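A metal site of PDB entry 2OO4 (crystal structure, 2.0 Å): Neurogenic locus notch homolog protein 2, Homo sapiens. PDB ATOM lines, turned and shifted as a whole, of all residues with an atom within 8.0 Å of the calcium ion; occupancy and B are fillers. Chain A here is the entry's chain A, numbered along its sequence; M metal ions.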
ATOM      1  N   TYR A  87      -0.092  16.180 -24.417  1.00  0.00           N
ATOM      2  CA  TYR A  87      -0.900  16.165 -23.193  1.00  0.00           C
ATOM      3  C   TYR A  87      -0.079  16.641 -21.986  1.00  0.00           C
ATOM      4  O   TYR A  87      -0.531  17.478 -21.210  1.00  0.00           O
ATOM      5  CB  TYR A  87      -1.444  14.766 -22.924  1.00  0.00           C
ATOM      6  CG  TYR A  87      -2.283  14.636 -21.670  1.00  0.00           C
ATOM      7  CD1 TYR A  87      -3.622  15.010 -21.666  1.00  0.00           C
ATOM      8  CD2 TYR A  87      -1.725  14.150 -20.483  1.00  0.00           C
ATOM      9  CE1 TYR A  87      -4.396  14.897 -20.508  1.00  0.00           C
ATOM     10  CE2 TYR A  87      -2.490  14.033 -19.326  1.00  0.00           C
ATOM     11  CZ  TYR A  87      -3.831  14.407 -19.344  1.00  0.00           C
ATOM     12  OH  TYR A  87      -4.597  14.296 -18.218  1.00  0.00           O
ATOM     13  N   CYS A  88       1.127  16.100 -21.853  1.00  0.00           N
ATOM     14  CA  CYS A  88       1.933  16.373 -20.680  1.00  0.00           C
ATOM     15  C   CYS A  88       2.439  17.825 -20.638  1.00  0.00           C
ATOM     16  O   CYS A  88       2.417  18.443 -19.578  1.00  0.00           O
ATOM     17  CB  CYS A  88       3.074  15.357 -20.540  1.00  0.00           C
ATOM     18  SG  CYS A  88       2.473  13.714 -20.004  1.00  0.00           S
ATOM     19  N   ALA A  89       2.838  18.360 -21.793  1.00  0.00           N
ATOM     20  CA  ALA A  89       3.255  19.773 -21.870  1.00  0.00           C
ATOM     21  C   ALA A  89       2.140  20.714 -21.372  1.00  0.00           C
ATOM     22  O   ALA A  89       2.403  21.609 -20.568  1.00  0.00           O
ATOM     23  CB  ALA A  89       3.685  20.157 -23.286  1.00  0.00           C
ATOM     24  N   ASP A  90       0.918  20.477 -21.830  1.00  0.00           N
ATOM     25  CA  ASP A  90      -0.241  21.309 -21.435  1.00  0.00           C
ATOM     26  C   ASP A  90      -0.626  21.143 -19.975  1.00  0.00           C
ATOM     27  O   ASP A  90      -1.253  22.034 -19.396  1.00  0.00           O
ATOM     28  CB  ASP A  90      -1.451  21.017 -22.333  1.00  0.00           C
ATOM     29  CG  ASP A  90      -1.358  21.685 -23.697  1.00  0.00           C
ATOM     30  OD1 ASP A  90      -0.331  22.339 -24.000  1.00  0.00           O
ATOM     31  OD2 ASP A  90      -2.312  21.543 -24.478  1.00  0.00           O
ATOM     32  N   HIS A  91      -0.272  20.013 -19.373  1.00  0.00           N
ATOM     33  CA  HIS A  91      -0.627  19.718 -17.983  1.00  0.00           C
ATOM     34  C   HIS A  91       0.554  19.840 -17.004  1.00  0.00           C
ATOM     35  O   HIS A  91       0.422  19.568 -15.810  1.00  0.00           O
ATOM     36  CB  HIS A  91      -1.302  18.346 -17.884  1.00  0.00           C
ATOM     37  CG  HIS A  91      -2.628  18.292 -18.568  1.00  0.00           C
ATOM     38  ND1 HIS A  91      -2.769  18.279 -19.935  1.00  0.00           N
ATOM     39  CD2 HIS A  91      -3.887  18.278 -18.060  1.00  0.00           C
ATOM     40  CE1 HIS A  91      -4.047  18.235 -20.250  1.00  0.00           C
ATOM     41  NE2 HIS A  91      -4.758  18.236 -19.129  1.00  0.00           N
ATOM     42  N   PHE A  92       1.702  20.293 -17.524  1.00  0.00           N
ATOM     43  CA  PHE A  92       2.911  20.475 -16.748  1.00  0.00           C
ATOM     44  C   PHE A  92       2.769  21.649 -15.791  1.00  0.00           C
ATOM     45  O   PHE A  92       2.430  22.763 -16.198  1.00  0.00           O
ATOM     46  CB  PHE A  92       4.080  20.709 -17.720  1.00  0.00           C
ATOM     47  CG  PHE A  92       5.405  20.997 -17.068  1.00  0.00           C
ATOM     48  CD1 PHE A  92       6.276  19.964 -16.768  1.00  0.00           C
ATOM     49  CD2 PHE A  92       5.797  22.306 -16.818  1.00  0.00           C
ATOM     50  CE1 PHE A  92       7.529  20.217 -16.209  1.00  0.00           C
ATOM     51  CE2 PHE A  92       7.041  22.583 -16.248  1.00  0.00           C
ATOM     52  CZ  PHE A  92       7.906  21.534 -15.935  1.00  0.00           C
ATOM     53  N   LYS A  93       3.050  21.399 -14.524  1.00  0.00           N
ATOM     54  CA  LYS A  93       2.970  22.430 -13.484  1.00  0.00           C
ATOM     55  C   LYS A  93       1.621  23.156 -13.511  1.00  0.00           C
ATOM     56  O   LYS A  93       1.550  24.376 -13.598  1.00  0.00           O
ATOM     57  CB  LYS A  93       4.151  23.399 -13.593  1.00  0.00           C
ATOM     58  CG  LYS A  93       4.722  23.839 -12.255  1.00  0.00           C
ATOM     59  CD  LYS A  93       5.732  24.976 -12.427  1.00  0.00           C
ATOM     60  CE  LYS A  93       6.263  25.466 -11.070  1.00  0.00           C
ATOM     61  NZ  LYS A  93       5.192  25.811 -10.073  1.00  0.00           N
ATOM     62  N   ASP A  94       0.532  22.390 -13.471  1.00  0.00           N
ATOM     63  CA  ASP A  94      -0.815  22.957 -13.486  1.00  0.00           C
ATOM     64  C   ASP A  94      -1.558  22.711 -12.165  1.00  0.00           C
ATOM     65  O   ASP A  94      -2.784  22.820 -12.097  1.00  0.00           O
ATOM     66  CB  ASP A  94      -1.621  22.439 -14.678  1.00  0.00           C
ATOM     67  CG  ASP A  94      -1.939  20.952 -14.591  1.00  0.00           C
ATOM     68  OD1 ASP A  94      -1.466  20.261 -13.660  1.00  0.00           O
ATOM     69  OD2 ASP A  94      -2.654  20.457 -15.480  1.00  0.00           O
ATOM     70  N   ASN A  95      -0.776  22.372 -11.125  1.00  0.00           N
ATOM     71  CA  ASN A  95      -1.287  22.113  -9.781  1.00  0.00           C
ATOM     72  C   ASN A  95      -2.251  20.923  -9.675  1.00  0.00           C
ATOM     73  O   ASN A  95      -3.118  20.893  -8.801  1.00  0.00           O
ATOM     74  CB  ASN A  95      -1.914  23.383  -9.174  1.00  0.00           C
ATOM     75  CG  ASN A  95      -0.898  24.495  -8.987  1.00  0.00           C
ATOM     76  OD1 ASN A  95       0.220  24.250  -8.542  1.00  0.00           O
ATOM     77  ND2 ASN A  95      -1.279  25.715  -9.336  1.00  0.00           N
ATOM     78  N   HIS A  96      -2.077  19.957 -10.560  1.00  0.00           N
ATOM     79  CA  HIS A  96      -2.853  18.719 -10.554  1.00  0.00           C
ATOM     80  C   HIS A  96      -1.925  17.583 -10.969  1.00  0.00           C
ATOM     81  O   HIS A  96      -1.247  17.674 -11.993  1.00  0.00           O
ATOM     82  CB  HIS A  96      -4.029  18.834 -11.529  1.00  0.00           C
ATOM     83  CG  HIS A  96      -4.903  17.613 -11.572  1.00  0.00           C
ATOM     84  ND1 HIS A  96      -6.006  17.459 -10.765  1.00  0.00           N
ATOM     85  CD2 HIS A  96      -4.833  16.500 -12.340  1.00  0.00           C
ATOM     86  CE1 HIS A  96      -6.576  16.292 -11.024  1.00  0.00           C
ATOM     87  NE2 HIS A  96      -5.881  15.693 -11.968  1.00  0.00           N
ATOM     88  N   CYS A  97      -1.887  16.515 -10.163  1.00  0.00           N
ATOM     89  CA  CYS A  97      -1.025  15.377 -10.465  1.00  0.00           C
ATOM     90  C   CYS A  97      -1.546  14.571 -11.650  1.00  0.00           C
ATOM     91  O   CYS A  97      -2.595  13.920 -11.560  1.00  0.00           O
ATOM     92  CB  CYS A  97      -0.858  14.471  -9.229  1.00  0.00           C
ATOM     93  SG  CYS A  97       0.106  12.949  -9.536  1.00  0.00           S
ATOM     94  N   ASN A  98      -0.825  14.634 -12.760  1.00  0.00           N
ATOM     95  CA  ASN A  98      -1.102  13.793 -13.920  1.00  0.00           C
ATOM     96  C   ASN A  98      -0.115  12.626 -13.884  1.00  0.00           C
ATOM     97  O   ASN A  98       1.070  12.800 -14.167  1.00  0.00           O
ATOM     98  CB  ASN A  98      -0.952  14.584 -15.218  1.00  0.00           C
ATOM     99  CG  ASN A  98      -1.922  15.751 -15.296  1.00  0.00           C
ATOM    100  OD1 ASN A  98      -3.081  15.588 -15.721  1.00  0.00           O
ATOM    101  ND2 ASN A  98      -1.466  16.926 -14.891  1.00  0.00           N
ATOM    102  N   GLN A  99      -0.607  11.447 -13.512  1.00  0.00           N
ATOM    103  CA  GLN A  99       0.274  10.299 -13.312  1.00  0.00           C
ATOM    104  C   GLN A  99       1.004   9.844 -14.573  1.00  0.00           C
ATOM    105  O   GLN A  99       2.169   9.463 -14.501  1.00  0.00           O
ATOM    106  CB  GLN A  99      -0.470   9.131 -12.641  1.00  0.00           C
ATOM    107  CG  GLN A  99      -0.565   9.243 -11.122  1.00  0.00           C
ATOM    108  CD  GLN A  99       0.798   9.348 -10.431  1.00  0.00           C
ATOM    109  OE1 GLN A  99       1.788   8.753 -10.877  1.00  0.00           O
ATOM    110  NE2 GLN A  99       0.849  10.085  -9.338  1.00  0.00           N
ATOM    111  N   CYS A 101       2.321  11.590 -16.626  1.00  0.00           N
ATOM    112  CA  CYS A 101       3.392  12.556 -16.895  1.00  0.00           C
ATOM    113  C   CYS A 101       4.431  12.560 -15.767  1.00  0.00           C
ATOM    114  O   CYS A 101       5.374  13.343 -15.784  1.00  0.00           O
ATOM    115  CB  CYS A 101       2.802  13.960 -17.023  1.00  0.00           C
ATOM    116  SG  CYS A 101       1.516  14.116 -18.260  1.00  0.00           S
ATOM    117  N   ASN A 102       4.210  11.697 -14.771  1.00  0.00           N
ATOM    118  CA  ASN A 102       5.057  11.661 -13.586  1.00  0.00           C
ATOM    119  C   ASN A 102       6.254  10.724 -13.782  1.00  0.00           C
ATOM    120  O   ASN A 102       6.323   9.654 -13.186  1.00  0.00           O
ATOM    121  CB  ASN A 102       4.232  11.246 -12.358  1.00  0.00           C
ATOM    122  CG  ASN A 102       5.007  11.381 -11.065  1.00  0.00           C
ATOM    123  OD1 ASN A 102       6.027  12.072 -10.994  1.00  0.00           O
ATOM    124  ND2 ASN A 102       4.520  10.718 -10.027  1.00  0.00           N
ATOM    125  N   TRP A 108       8.600  14.906 -14.475  1.00  0.00           N
ATOM    126  CA  TRP A 108       7.776  14.615 -13.287  1.00  0.00           C
ATOM    127  C   TRP A 108       6.591  15.561 -13.120  1.00  0.00           C
ATOM    128  O   TRP A 108       6.299  16.004 -12.000  1.00  0.00           O
ATOM    129  CB  TRP A 108       8.611  14.576 -11.993  1.00  0.00           C
ATOM    130  CG  TRP A 108       9.678  13.520 -11.938  1.00  0.00           C
ATOM    131  CD1 TRP A 108       9.541  12.247 -11.478  1.00  0.00           C
ATOM    132  CD2 TRP A 108      11.050  13.650 -12.353  1.00  0.00           C
ATOM    133  NE1 TRP A 108      10.730  11.568 -11.582  1.00  0.00           N
ATOM    134  CE2 TRP A 108      11.676  12.409 -12.118  1.00  0.00           C
ATOM    135  CE3 TRP A 108      11.804  14.700 -12.912  1.00  0.00           C
ATOM    136  CZ2 TRP A 108      13.033  12.184 -12.406  1.00  0.00           C
ATOM    137  CZ3 TRP A 108      13.148  14.471 -13.203  1.00  0.00           C
ATOM    138  CH2 TRP A 108      13.753  13.225 -12.939  1.00  0.00           C
ATOM    139  N   ASP A 109       5.928  15.861 -14.231  1.00  0.00           N
ATOM    140  CA  ASP A 109       4.711  16.692 -14.236  1.00  0.00           C
ATOM    141  C   ASP A 109       4.953  18.049 -13.556  1.00  0.00           C
ATOM    142  O   ASP A 109       4.035  18.625 -12.988  1.00  0.00           O
ATOM    143  CB  ASP A 109       3.560  15.923 -13.556  1.00  0.00           C
ATOM    144  CG  ASP A 109       2.209  16.574 -13.766  1.00  0.00           C
ATOM    145  OD1 ASP A 109       2.033  17.313 -14.760  1.00  0.00           O
ATOM    146  OD2 ASP A 109       1.307  16.367 -12.927  1.00  0.00           O
ATOM    147  N   GLY A 110       6.193  18.532 -13.604  1.00  0.00           N
ATOM    148  CA  GLY A 110       6.554  19.814 -13.024  1.00  0.00           C
ATOM    149  C   GLY A 110       6.394  19.867 -11.518  1.00  0.00           C
ATOM    150  O   GLY A 110       6.128  20.930 -10.967  1.00  0.00           O
ATOM    151  N   LEU A 111       6.549  18.712 -10.875  1.00  0.00           N
ATOM    152  CA  LEU A 111       6.398  18.521  -9.420  1.00  0.00           C
ATOM    153  C   LEU A 111       4.943  18.582  -8.900  1.00  0.00           C
ATOM    154  O   LEU A 111       4.725  18.676  -7.684  1.00  0.00           O
ATOM    155  CB  LEU A 111       7.345  19.414  -8.610  1.00  0.00           C
ATOM    156  CG  LEU A 111       8.848  19.232  -8.892  1.00  0.00           C
ATOM    157  CD1 LEU A 111       9.665  20.238  -8.132  1.00  0.00           C
ATOM    158  CD2 LEU A 111       9.330  17.798  -8.601  1.00  0.00           C
ATOM    159  N   ASP A 112       3.962  18.507  -9.797  1.00  0.00           N
ATOM    160  CA  ASP A 112       2.554  18.464  -9.389  1.00  0.00           C
ATOM    161  C   ASP A 112       2.207  17.238  -8.530  1.00  0.00           C
ATOM    162  O   ASP A 112       1.276  17.279  -7.742  1.00  0.00           O
ATOM    163  CB  ASP A 112       1.639  18.483 -10.613  1.00  0.00           C
ATOM    164  CG  ASP A 112       1.615  19.808 -11.325  1.00  0.00           C
ATOM    165  OD1 ASP A 112       2.012  20.849 -10.758  1.00  0.00           O
ATOM    166  OD2 ASP A 112       1.156  19.807 -12.491  1.00  0.00           O
ATOM    167  N   CYS A 113       2.959  16.145  -8.711  1.00  0.00           N
ATOM    168  CA  CYS A 113       2.723  14.898  -7.971  1.00  0.00           C
ATOM    169  C   CYS A 113       3.590  14.774  -6.714  1.00  0.00           C
ATOM    170  O   CYS A 113       3.566  13.746  -6.031  1.00  0.00           O
ATOM    171  CB  CYS A 113       2.952  13.686  -8.879  1.00  0.00           C
ATOM    172  SG  CYS A 113       1.866  13.612 -10.315  1.00  0.00           S
ATOM    173  N   ARG A 142       6.303  28.314 -17.949  1.00  0.00           N
ATOM    174  CA  ARG A 142       6.144  26.869 -17.822  1.00  0.00           C
ATOM    175  C   ARG A 142       6.861  26.098 -18.913  1.00  0.00           C
ATOM    176  O   ARG A 142       7.562  25.134 -18.635  1.00  0.00           O
ATOM    177  CB  ARG A 142       4.678  26.483 -17.722  1.00  0.00           C
ATOM    178  CG  ARG A 142       4.107  26.751 -16.331  1.00  0.00           C
ATOM    179  CD  ARG A 142       2.609  26.729 -16.304  1.00  0.00           C
ATOM    180  NE  ARG A 142       2.056  25.452 -16.726  1.00  0.00           N
ATOM    181  CZ  ARG A 142       1.259  25.285 -17.780  1.00  0.00           C
ATOM    182  NH1 ARG A 142       0.922  26.325 -18.535  1.00  0.00           N
ATOM    183  NH2 ARG A 142       0.810  24.078 -18.088  1.00  0.00           N
HETATM  184 CA    CA M   1       0.019  18.339 -13.862  1.00  0.00          CA
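SG of Cys 97 forms a disulfide with SG of Cys 113.
The backbone carbonyl oxygen of Cys 101 sits at hydrogen-bond distance from the backbone NH of Asp 109 (3.0 Å).
SG of Cys 101 forms a disulfide with SG of Cys 88 (2.0 Å).
OD2 of Asp 112 sits close to N of Lys 93 (3.2 Å).
The side-chain amide oxygen (OD1) of Asn 98 is in hydrogen-bond range of the side-chain hydroxyl (OH) of Tyr 87.
The backbone carbonyl oxygen (O) of Asp 109 sits at hydrogen-bond distance from the backbone NH (N) of Lys 93 (3.3 Å).
A ring nitrogen (ND1) of His 91 lies within hydrogen-bond range of the backbone carbonyl oxygen (O) of Tyr 87 (2.7 Å).
The backbone NH (N) of Asn 95 is in hydrogen-bond range of the side-chain carboxylate (OD1) of Asp 112.
The calcium ion is bound by ND2 of Asn 98 (2.3 Å), OD2 of Asp 112 (2.3 Å), O of His 91 (2.3 Å), O of His 96 (2.4 Å), OD1 of Asp 109 (2.4 Å), OD1 of Asp 94 (2.4 Å) and OD2 of Asp 109 (2.5 Å).
The calcium ion has seven donor atoms within binding distance.
Six residues have an atom within 4 Å of the calcium ion: His 91, Asp 94, His 96, Asn 98, Asp 109 and Asp 112.
Along chain A the residues within 4 Å of the calcium ion span positions 91 to 112.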
